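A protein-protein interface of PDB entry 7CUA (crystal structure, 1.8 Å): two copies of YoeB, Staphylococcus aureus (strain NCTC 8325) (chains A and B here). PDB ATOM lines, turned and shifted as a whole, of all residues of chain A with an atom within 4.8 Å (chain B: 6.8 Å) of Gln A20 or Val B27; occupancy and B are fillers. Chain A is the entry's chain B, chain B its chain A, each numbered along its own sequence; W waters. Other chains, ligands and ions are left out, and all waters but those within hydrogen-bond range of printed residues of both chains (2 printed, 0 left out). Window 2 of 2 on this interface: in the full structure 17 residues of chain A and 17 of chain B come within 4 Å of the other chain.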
ATOM      1  N   TYR A  16     -20.971 -14.494   9.258  1.00  0.00           N
ATOM      2  CA  TYR A  16     -22.255 -13.823   9.096  1.00  0.00           C
ATOM      3  C   TYR A  16     -22.131 -12.328   9.357  1.00  0.00           C
ATOM      4  O   TYR A  16     -22.680 -11.511   8.608  1.00  0.00           O
ATOM      5  CB  TYR A  16     -23.262 -14.477  10.043  1.00  0.00           C
ATOM      6  CG  TYR A  16     -24.718 -14.141   9.831  1.00  0.00           C
ATOM      7  CD1 TYR A  16     -25.392 -14.531   8.679  1.00  0.00           C
ATOM      8  CD2 TYR A  16     -25.434 -13.476  10.813  1.00  0.00           C
ATOM      9  CE1 TYR A  16     -26.736 -14.236   8.504  1.00  0.00           C
ATOM     10  CE2 TYR A  16     -26.775 -13.183  10.652  1.00  0.00           C
ATOM     11  CZ  TYR A  16     -27.422 -13.562   9.500  1.00  0.00           C
ATOM     12  OH  TYR A  16     -28.759 -13.262   9.351  1.00  0.00           O
ATOM     13  N   LYS A  17     -21.401 -11.948  10.408  1.00  0.00           N
ATOM     14  CA  LYS A  17     -21.231 -10.531  10.708  1.00  0.00           C
ATOM     15  C   LYS A  17     -20.376  -9.844   9.649  1.00  0.00           C
ATOM     16  O   LYS A  17     -20.620  -8.681   9.303  1.00  0.00           O
ATOM     17  CB  LYS A  17     -20.614 -10.356  12.096  1.00  0.00           C
ATOM     18  CG  LYS A  17     -21.562 -10.695  13.233  1.00  0.00           C
ATOM     19  CD  LYS A  17     -20.959 -10.326  14.586  1.00  0.00           C
ATOM     20  CE  LYS A  17     -19.728 -11.164  14.886  1.00  0.00           C
ATOM     21  NZ  LYS A  17     -18.972 -10.663  16.070  1.00  0.00           N
ATOM     22  N   TYR A  18     -19.370 -10.549   9.127  1.00  0.00           N
ATOM     23  CA  TYR A  18     -18.579 -10.026   8.017  1.00  0.00           C
ATOM     24  C   TYR A  18     -19.471  -9.649   6.839  1.00  0.00           C
ATOM     25  O   TYR A  18     -19.336  -8.562   6.263  1.00  0.00           O
ATOM     26  CB  TYR A  18     -17.535 -11.063   7.600  1.00  0.00           C
ATOM     27  CG  TYR A  18     -16.833 -10.764   6.290  1.00  0.00           C
ATOM     28  CD1 TYR A  18     -15.718  -9.938   6.249  1.00  0.00           C
ATOM     29  CD2 TYR A  18     -17.278 -11.323   5.097  1.00  0.00           C
ATOM     30  CE1 TYR A  18     -15.070  -9.667   5.055  1.00  0.00           C
ATOM     31  CE2 TYR A  18     -16.637 -11.058   3.899  1.00  0.00           C
ATOM     32  CZ  TYR A  18     -15.534 -10.230   3.883  1.00  0.00           C
ATOM     33  OH  TYR A  18     -14.895  -9.968   2.691  1.00  0.00           O
ATOM     34  N   PHE A  19     -20.392 -10.541   6.464  1.00  0.00           N
ATOM     35  CA  PHE A  19     -21.289 -10.257   5.351  1.00  0.00           C
ATOM     36  C   PHE A  19     -22.257  -9.125   5.683  1.00  0.00           C
ATOM     37  O   PHE A  19     -22.637  -8.358   4.791  1.00  0.00           O
ATOM     38  CB  PHE A  19     -22.059 -11.524   4.960  1.00  0.00           C
ATOM     39  CG  PHE A  19     -21.210 -12.589   4.310  1.00  0.00           C
ATOM     40  CD1 PHE A  19     -20.337 -12.274   3.279  1.00  0.00           C
ATOM     41  CD2 PHE A  19     -21.295 -13.908   4.727  1.00  0.00           C
ATOM     42  CE1 PHE A  19     -19.563 -13.257   2.679  1.00  0.00           C
ATOM     43  CE2 PHE A  19     -20.524 -14.896   4.131  1.00  0.00           C
ATOM     44  CZ  PHE A  19     -19.658 -14.569   3.105  1.00  0.00           C
ATOM     45  N   GLN A  20     -22.675  -9.009   6.949  1.00  0.00           N
ATOM     46  CA  GLN A  20     -23.518  -7.882   7.345  1.00  0.00           C
ATOM     47  C   GLN A  20     -22.855  -6.557   6.989  1.00  0.00           C
ATOM     48  O   GLN A  20     -23.525  -5.609   6.564  1.00  0.00           O
ATOM     49  CB  GLN A  20     -23.806  -7.931   8.845  1.00  0.00           C
ATOM     50  CG  GLN A  20     -24.755  -9.029   9.287  1.00  0.00           C
ATOM     51  CD  GLN A  20     -24.851  -9.123  10.799  1.00  0.00           C
ATOM     52  OE1 GLN A  20     -24.253  -8.321  11.522  1.00  0.00           O
ATOM     53  NE2 GLN A  20     -25.585 -10.113  11.284  1.00  0.00           N
ATOM     54  N   GLN A  21     -21.537  -6.481   7.158  1.00  0.00           N
ATOM     55  CA  GLN A  21     -20.766  -5.271   6.908  1.00  0.00           C
ATOM     56  C   GLN A  21     -20.344  -5.112   5.454  1.00  0.00           C
ATOM     57  O   GLN A  21     -20.254  -3.979   4.966  1.00  0.00           O
ATOM     58  CB  GLN A  21     -19.510  -5.266   7.786  1.00  0.00           C
ATOM     59  CG  GLN A  21     -19.760  -4.915   9.242  1.00  0.00           C
ATOM     60  CD  GLN A  21     -19.507  -3.448   9.533  1.00  0.00           C
ATOM     61  OE1 GLN A  21     -20.431  -2.694   9.840  1.00  0.00           O
ATOM     62  NE2 GLN A  21     -18.248  -3.035   9.435  1.00  0.00           N
ATOM     63  N   ASN A  22     -20.081  -6.214   4.748  1.00  0.00           N
ATOM     64  CA  ASN A  22     -19.389  -6.154   3.470  1.00  0.00           C
ATOM     65  C   ASN A  22     -20.154  -6.739   2.294  1.00  0.00           C
ATOM     66  O   ASN A  22     -19.798  -6.439   1.151  1.00  0.00           O
ATOM     67  CB  ASN A  22     -18.031  -6.866   3.570  1.00  0.00           C
ATOM     68  CG  ASN A  22     -17.129  -6.235   4.602  1.00  0.00           C
ATOM     69  OD1 ASN A  22     -16.767  -6.863   5.597  1.00  0.00           O
ATOM     70  ND2 ASN A  22     -16.767  -4.976   4.379  1.00  0.00           N
ATOM     71  N   LYS A  24     -24.236  -7.525   2.028  1.00  0.00           N
ATOM     72  CA  LYS A  24     -25.571  -7.764   2.564  1.00  0.00           C
ATOM     73  C   LYS A  24     -26.394  -8.696   1.689  1.00  0.00           C
ATOM     74  O   LYS A  24     -27.335  -9.321   2.188  1.00  0.00           O
ATOM     75  CB  LYS A  24     -26.295  -6.430   2.741  1.00  0.00           C
ATOM     76  CG  LYS A  24     -25.589  -5.500   3.710  1.00  0.00           C
ATOM     77  CD  LYS A  24     -26.140  -4.084   3.652  1.00  0.00           C
ATOM     78  CE  LYS A  24     -25.381  -3.178   4.612  1.00  0.00           C
ATOM     79  NZ  LYS A  24     -25.724  -1.740   4.436  1.00  0.00           N
ATOM     80  N   VAL A  27     -26.030 -12.032   3.206  1.00  0.00           N
ATOM     81  CA  VAL A  27     -26.851 -12.190   4.406  1.00  0.00           C
ATOM     82  C   VAL A  27     -28.275 -12.556   4.022  1.00  0.00           C
ATOM     83  O   VAL A  27     -28.878 -13.475   4.592  1.00  0.00           O
ATOM     84  CB  VAL A  27     -26.822 -10.910   5.262  1.00  0.00           C
ATOM     85  CG1 VAL A  27     -27.833 -11.008   6.404  1.00  0.00           C
ATOM     86  CG2 VAL A  27     -25.434 -10.670   5.813  1.00  0.00           C
ATOM     87  N   ASP B  15     -36.606 -10.985  15.390  1.00  0.00           N
ATOM     88  CA  ASP B  15     -36.219  -9.653  15.855  1.00  0.00           C
ATOM     89  C   ASP B  15     -34.916  -9.200  15.210  1.00  0.00           C
ATOM     90  O   ASP B  15     -34.786  -8.045  14.788  1.00  0.00           O
ATOM     91  CB  ASP B  15     -36.054  -9.638  17.378  1.00  0.00           C
ATOM     92  CG  ASP B  15     -37.328 -10.001  18.128  1.00  0.00           C
ATOM     93  OD1 ASP B  15     -38.428  -9.935  17.544  1.00  0.00           O
ATOM     94  OD2 ASP B  15     -37.214 -10.344  19.325  1.00  0.00           O
ATOM     95  N   TYR B  16     -33.929 -10.096  15.150  1.00  0.00           N
ATOM     96  CA  TYR B  16     -32.613  -9.742  14.627  1.00  0.00           C
ATOM     97  C   TYR B  16     -32.693  -9.368  13.152  1.00  0.00           C
ATOM     98  O   TYR B  16     -32.092  -8.376  12.718  1.00  0.00           O
ATOM     99  CB  TYR B  16     -31.666 -10.923  14.857  1.00  0.00           C
ATOM    100  CG  TYR B  16     -30.184 -10.683  14.647  1.00  0.00           C
ATOM    101  CD1 TYR B  16     -29.447  -9.899  15.529  1.00  0.00           C
ATOM    102  CD2 TYR B  16     -29.510 -11.301  13.602  1.00  0.00           C
ATOM    103  CE1 TYR B  16     -28.081  -9.703  15.345  1.00  0.00           C
ATOM    104  CE2 TYR B  16     -28.150 -11.118  13.411  1.00  0.00           C
ATOM    105  CZ  TYR B  16     -27.441 -10.321  14.286  1.00  0.00           C
ATOM    106  OH  TYR B  16     -26.092 -10.145  14.087  1.00  0.00           O
ATOM    107  N   LYS B  17     -33.448 -10.139  12.366  1.00  0.00           N
ATOM    108  CA  LYS B  17     -33.640  -9.800  10.960  1.00  0.00           C
ATOM    109  C   LYS B  17     -34.451  -8.519  10.798  1.00  0.00           C
ATOM    110  O   LYS B  17     -34.227  -7.761   9.845  1.00  0.00           O
ATOM    111  CB  LYS B  17     -34.323 -10.958  10.231  1.00  0.00           C
ATOM    112  CG  LYS B  17     -33.428 -12.192  10.061  1.00  0.00           C
ATOM    113  CD  LYS B  17     -34.071 -13.219   9.142  1.00  0.00           C
ATOM    114  CE  LYS B  17     -35.308 -13.842   9.776  1.00  0.00           C
ATOM    115  NZ  LYS B  17     -35.906 -14.892   8.891  1.00  0.00           N
ATOM    116  N   TYR B  18     -35.401  -8.273  11.702  1.00  0.00           N
ATOM    117  CA  TYR B  18     -36.134  -7.011  11.678  1.00  0.00           C
ATOM    118  C   TYR B  18     -35.185  -5.825  11.778  1.00  0.00           C
ATOM    119  O   TYR B  18     -35.333  -4.834  11.051  1.00  0.00           O
ATOM    120  CB  TYR B  18     -37.161  -6.978  12.813  1.00  0.00           C
ATOM    121  CG  TYR B  18     -37.830  -5.631  12.992  1.00  0.00           C
ATOM    122  CD1 TYR B  18     -37.268  -4.653  13.810  1.00  0.00           C
ATOM    123  CD2 TYR B  18     -39.019  -5.337  12.343  1.00  0.00           C
ATOM    124  CE1 TYR B  18     -37.881  -3.417  13.973  1.00  0.00           C
ATOM    125  CE2 TYR B  18     -39.637  -4.106  12.502  1.00  0.00           C
ATOM    126  CZ  TYR B  18     -39.063  -3.154  13.316  1.00  0.00           C
ATOM    127  OH  TYR B  18     -39.681  -1.929  13.468  1.00  0.00           O
ATOM    128  N   PHE B  19     -34.205  -5.905  12.677  1.00  0.00           N
ATOM    129  CA  PHE B  19     -33.228  -4.827  12.788  1.00  0.00           C
ATOM    130  C   PHE B  19     -32.282  -4.786  11.596  1.00  0.00           C
ATOM    131  O   PHE B  19     -31.821  -3.702  11.218  1.00  0.00           O
ATOM    132  CB  PHE B  19     -32.451  -4.958  14.092  1.00  0.00           C
ATOM    133  CG  PHE B  19     -33.278  -4.647  15.304  1.00  0.00           C
ATOM    134  CD1 PHE B  19     -34.046  -3.490  15.353  1.00  0.00           C
ATOM    135  CD2 PHE B  19     -33.322  -5.523  16.376  1.00  0.00           C
ATOM    136  CE1 PHE B  19     -34.822  -3.200  16.461  1.00  0.00           C
ATOM    137  CE2 PHE B  19     -34.094  -5.243  17.485  1.00  0.00           C
ATOM    138  CZ  PHE B  19     -34.847  -4.076  17.530  1.00  0.00           C
ATOM    139  N   GLN B  20     -31.976  -5.940  10.992  1.00  0.00           N
ATOM    140  CA  GLN B  20     -31.202  -5.927   9.753  1.00  0.00           C
ATOM    141  C   GLN B  20     -31.909  -5.109   8.682  1.00  0.00           C
ATOM    142  O   GLN B  20     -31.266  -4.386   7.912  1.00  0.00           O
ATOM    143  CB  GLN B  20     -30.967  -7.354   9.250  1.00  0.00           C
ATOM    144  CG  GLN B  20     -30.057  -8.204  10.124  1.00  0.00           C
ATOM    145  CD  GLN B  20     -29.962  -9.650   9.640  1.00  0.00           C
ATOM    146  OE1 GLN B  20     -30.556 -10.025   8.624  1.00  0.00           O
ATOM    147  NE2 GLN B  20     -29.212 -10.467  10.369  1.00  0.00           N
ATOM    148  N   GLN B  21     -33.238  -5.196   8.634  1.00  0.00           N
ATOM    149  CA  GLN B  21     -33.998  -4.496   7.610  1.00  0.00           C
ATOM    150  C   GLN B  21     -34.261  -3.038   7.979  1.00  0.00           C
ATOM    151  O   GLN B  21     -34.415  -2.198   7.085  1.00  0.00           O
ATOM    152  CB  GLN B  21     -35.312  -5.237   7.361  1.00  0.00           C
ATOM    153  CG  GLN B  21     -36.169  -4.675   6.239  1.00  0.00           C
ATOM    154  CD  GLN B  21     -37.296  -5.617   5.849  1.00  0.00           C
ATOM    155  OE1 GLN B  21     -38.435  -5.463   6.296  1.00  0.00           O
ATOM    156  NE2 GLN B  21     -36.979  -6.603   5.016  1.00  0.00           N
ATOM    157  N   ASP B  23     -32.715  -1.073  11.055  1.00  0.00           N
ATOM    158  CA  ASP B  23     -31.783  -0.234  11.820  1.00  0.00           C
ATOM    159  C   ASP B  23     -30.500  -1.044  12.029  1.00  0.00           C
ATOM    160  O   ASP B  23     -30.366  -1.767  13.017  1.00  0.00           O
ATOM    161  CB  ASP B  23     -32.385   0.209  13.141  1.00  0.00           C
ATOM    162  CG  ASP B  23     -31.566   1.293  13.840  1.00  0.00           C
ATOM    163  OD1 ASP B  23     -30.365   1.450  13.544  1.00  0.00           O
ATOM    164  OD2 ASP B  23     -32.127   1.983  14.714  1.00  0.00           O
ATOM    165  N   LYS B  24     -29.560  -0.893  11.097  1.00  0.00           N
ATOM    166  CA  LYS B  24     -28.350  -1.699  11.156  1.00  0.00           C
ATOM    167  C   LYS B  24     -27.465  -1.335  12.342  1.00  0.00           C
ATOM    168  O   LYS B  24     -26.654  -2.165  12.765  1.00  0.00           O
ATOM    169  CB  LYS B  24     -27.592  -1.584   9.835  1.00  0.00           C
ATOM    170  CG  LYS B  24     -28.382  -2.159   8.657  1.00  0.00           C
ATOM    171  CD  LYS B  24     -27.650  -1.983   7.330  1.00  0.00           C
ATOM    172  CE  LYS B  24     -28.591  -2.218   6.154  1.00  0.00           C
ATOM    173  NZ  LYS B  24     -29.127  -3.609   6.136  1.00  0.00           N
ATOM    174  N   LYS B  25     -27.619  -0.134  12.911  1.00  0.00           N
ATOM    175  CA  LYS B  25     -26.883   0.181  14.132  1.00  0.00           C
ATOM    176  C   LYS B  25     -27.366  -0.649  15.312  1.00  0.00           C
ATOM    177  O   LYS B  25     -26.591  -0.918  16.237  1.00  0.00           O
ATOM    178  CB  LYS B  25     -26.996   1.668  14.455  1.00  0.00           C
ATOM    179  CG  LYS B  25     -26.224   2.560  13.496  1.00  0.00           C
ATOM    180  CD  LYS B  25     -25.885   3.913  14.115  1.00  0.00           C
ATOM    181  CE  LYS B  25     -26.933   4.366  15.124  1.00  0.00           C
ATOM    182  NZ  LYS B  25     -26.541   4.051  16.535  1.00  0.00           N
ATOM    183  N   MET B  26     -28.642  -1.045  15.309  1.00  0.00           N
ATOM    184  CA  MET B  26     -29.139  -1.931  16.357  1.00  0.00           C
ATOM    185  C   MET B  26     -28.542  -3.327  16.227  1.00  0.00           C
ATOM    186  O   MET B  26     -28.284  -3.991  17.238  1.00  0.00           O
ATOM    187  CB  MET B  26     -30.664  -1.985  16.318  1.00  0.00           C
ATOM    188  CG  MET B  26     -31.308  -0.653  16.629  1.00  0.00           C
ATOM    189  SD  MET B  26     -31.378  -0.379  18.407  1.00  0.00           S
ATOM    190  CE  MET B  26     -32.823  -1.332  18.822  1.00  0.00           C
ATOM    191  N   VAL B  27     -28.322  -3.792  14.995  1.00  0.00           N
ATOM    192  CA  VAL B  27     -27.632  -5.065  14.794  1.00  0.00           C
ATOM    193  C   VAL B  27     -26.222  -4.992  15.370  1.00  0.00           C
ATOM    194  O   VAL B  27     -25.769  -5.902  16.073  1.00  0.00           O
ATOM    195  CB  VAL B  27     -27.619  -5.444  13.301  1.00  0.00           C
ATOM    196  CG1 VAL B  27     -26.899  -6.785  13.084  1.00  0.00           C
ATOM    197  CG2 VAL B  27     -29.038  -5.516  12.756  1.00  0.00           C
ATOM    198  N   LYS B  28     -25.513  -3.892  15.094  1.00  0.00           N
ATOM    199  CA  LYS B  28     -24.161  -3.726  15.626  1.00  0.00           C
ATOM    200  C   LYS B  28     -24.148  -3.783  17.148  1.00  0.00           C
ATOM    201  O   LYS B  28     -23.291  -4.446  17.745  1.00  0.00           O
ATOM    202  CB  LYS B  28     -23.565  -2.403  15.146  1.00  0.00           C
ATOM    203  CG  LYS B  28     -22.723  -2.522  13.897  1.00  0.00           C
ATOM    204  CD  LYS B  28     -23.583  -2.750  12.680  1.00  0.00           C
ATOM    205  N   LYS B  29     -25.088  -3.086  17.790  1.00  0.00           N
ATOM    206  CA  LYS B  29     -25.138  -3.080  19.249  1.00  0.00           C
ATOM    207  C   LYS B  29     -25.397  -4.478  19.796  1.00  0.00           C
ATOM    208  O   LYS B  29     -24.750  -4.905  20.761  1.00  0.00           O
ATOM    209  CB  LYS B  29     -26.211  -2.108  19.730  1.00  0.00           C
ATOM    210  CG  LYS B  29     -26.538  -2.197  21.216  1.00  0.00           C
ATOM    211  CD  LYS B  29     -25.321  -1.918  22.091  1.00  0.00           C
ATOM    212  CE  LYS B  29     -24.819  -0.493  21.924  1.00  0.00           C
ATOM    213  NZ  LYS B  29     -23.774  -0.170  22.944  1.00  0.00           N
ATOM    214  N   ILE B  30     -26.344  -5.203  19.195  1.00  0.00           N
ATOM    215  CA  ILE B  30     -26.590  -6.590  19.592  1.00  0.00           C
ATOM    216  C   ILE B  30     -25.314  -7.416  19.460  1.00  0.00           C
ATOM    217  O   ILE B  30     -24.952  -8.178  20.364  1.00  0.00           O
ATOM    218  CB  ILE B  30     -27.743  -7.191  18.765  1.00  0.00           C
ATOM    219  CG1 ILE B  30     -29.065  -6.509  19.141  1.00  0.00           C
ATOM    220  CG2 ILE B  30     -27.836  -8.707  18.973  1.00  0.00           C
ATOM    221  CD1 ILE B  30     -30.198  -6.772  18.165  1.00  0.00           C
ATOM    222  N   ASN B  31     -24.610  -7.275  18.334  1.00  0.00           N
ATOM    223  CA  ASN B  31     -23.374  -8.034  18.163  1.00  0.00           C
ATOM    224  C   ASN B  31     -22.358  -7.670  19.241  1.00  0.00           C
ATOM    225  O   ASN B  31     -21.629  -8.537  19.736  1.00  0.00           O
ATOM    226  CB  ASN B  31     -22.786  -7.797  16.771  1.00  0.00           C
ATOM    227  CG  ASN B  31     -23.689  -8.301  15.660  1.00  0.00           C
ATOM    228  OD1 ASN B  31     -24.614  -9.080  15.893  1.00  0.00           O
ATOM    229  ND2 ASN B  31     -23.417  -7.863  14.438  1.00  0.00           N
ATOM    230  N   GLU B  32     -22.308  -6.393  19.628  1.00  0.00           N
ATOM    231  CA  GLU B  32     -21.367  -5.978  20.664  1.00  0.00           C
ATOM    232  C   GLU B  32     -21.749  -6.561  22.017  1.00  0.00           C
ATOM    233  O   GLU B  32     -20.876  -6.978  22.787  1.00  0.00           O
ATOM    234  CB  GLU B  32     -21.298  -4.453  20.740  1.00  0.00           C
ATOM    235  CG  GLU B  32     -20.571  -3.817  19.564  1.00  0.00           C
ATOM    236  CD  GLU B  32     -20.544  -2.304  19.641  1.00  0.00           C
ATOM    237  N   ILE B  64     -30.190  -2.762  24.628  1.00  0.00           N
ATOM    238  CA  ILE B  64     -29.796  -2.477  23.252  1.00  0.00           C
ATOM    239  C   ILE B  64     -29.945  -0.976  23.033  1.00  0.00           C
ATOM    240  O   ILE B  64     -28.988  -0.292  22.650  1.00  0.00           O
ATOM    241  CB  ILE B  64     -30.641  -3.282  22.247  1.00  0.00           C
ATOM    242  CG1 ILE B  64     -30.464  -4.786  22.486  1.00  0.00           C
ATOM    243  CG2 ILE B  64     -30.259  -2.936  20.820  1.00  0.00           C
ATOM    244  CD1 ILE B  64     -31.443  -5.633  21.699  1.00  0.00           C
HETATM  245  O   HOH W   1     -23.269  -5.773  11.673  1.00  0.00           O
HETATM  246  O   HOH W   2     -20.975 -10.883  18.338  1.00  0.00           O
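The backbone carbonyl oxygen (O) of Gln B20 sits at hydrogen-bond distance from the side-chain amino group (NZ) of Lys B24, at 2.9 Å.
The backbone carbonyl oxygen (O) of Val B27 lies close to the side-chain amide oxygen (OD1) of Asn B31 (3.4 Å).
OH of Tyr B16 sits at hydrogen-bond distance from OD1 of Asn B31 (2.6 Å).
N of Lys A24 is in hydrogen-bond range of O of Phe A19, at 3.3 Å.
NE2 of Gln A20 lies within hydrogen-bond range of OH of Tyr B16, 2.8 Å away.
The side-chain amide nitrogen (ND2) of Asn B31 is in hydrogen-bond range of the side-chain amide oxygen (OE1) of Gln A20, at 3.1 Å.
NE2 of Gln B20 lies within hydrogen-bond range of OH of Tyr A16 (3.0 Å).
CE2 of Tyr B16 touches CE2 of Tyr A16 (3.7 Å).
Asn B31 touches Lys A17.
NE2 of Gln A20 touches NE2 of Gln B20, 3.8 Å away.
Val B27 touches Gln A20.
NZ of Lys A24 touches CE of Lys B24 (3.4 Å).
Val A27 touches Gln B20 (CG1 to OE1, 3.6 Å).
Of the 18 printed residues of chain B, 5 touch a printed residue of chain A.
Of the 9 printed residues of chain A, 5 touch a printed residue of chain B.
Among the printed residues, no Asp or Glu carboxylate lies within 4 Å of a Lys or Arg side-chain nitrogen of the other chain.
Tyr A16 touches its own counterpart, Tyr B16.
Tyr A16 touches Gln B20, and with the chains exchanged Gln A20 touches Tyr B16.
Gln A20 touches Val B27, and with the chains exchanged Val A27 touches Gln B20.
Lys A24 touches its own counterpart, Lys B24.
8 positions are printed for both chains.
Of the 9 pairs that touch across the chains among the printed residues, 7 have their exchanged pair printed and touching as well.
Printed residues of chain B within 4 Å of Val A27: Gln B20.
Of the printed residues of chain A, Gln B20 touches Tyr A16, Gln A20 and Val A27.
Of chain A, only Gln A20 (3.4 Å) comes within 4 Å of Val B27.
The nearest printed residue of chain A that does not touch Val B27 is Lys A17 (6.6 Å).
The nearest printed residue of chain A that does not touch Tyr B16 is Lys A17 (4.6 Å).
Water W1 bridges OE1 of Gln A20 (2.7 Å) and ND2 of Asn B31 (3.5 Å).
Water W2 bridges O of Asn B31 (2.8 Å) and NZ of Lys A17 (3.0 Å).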
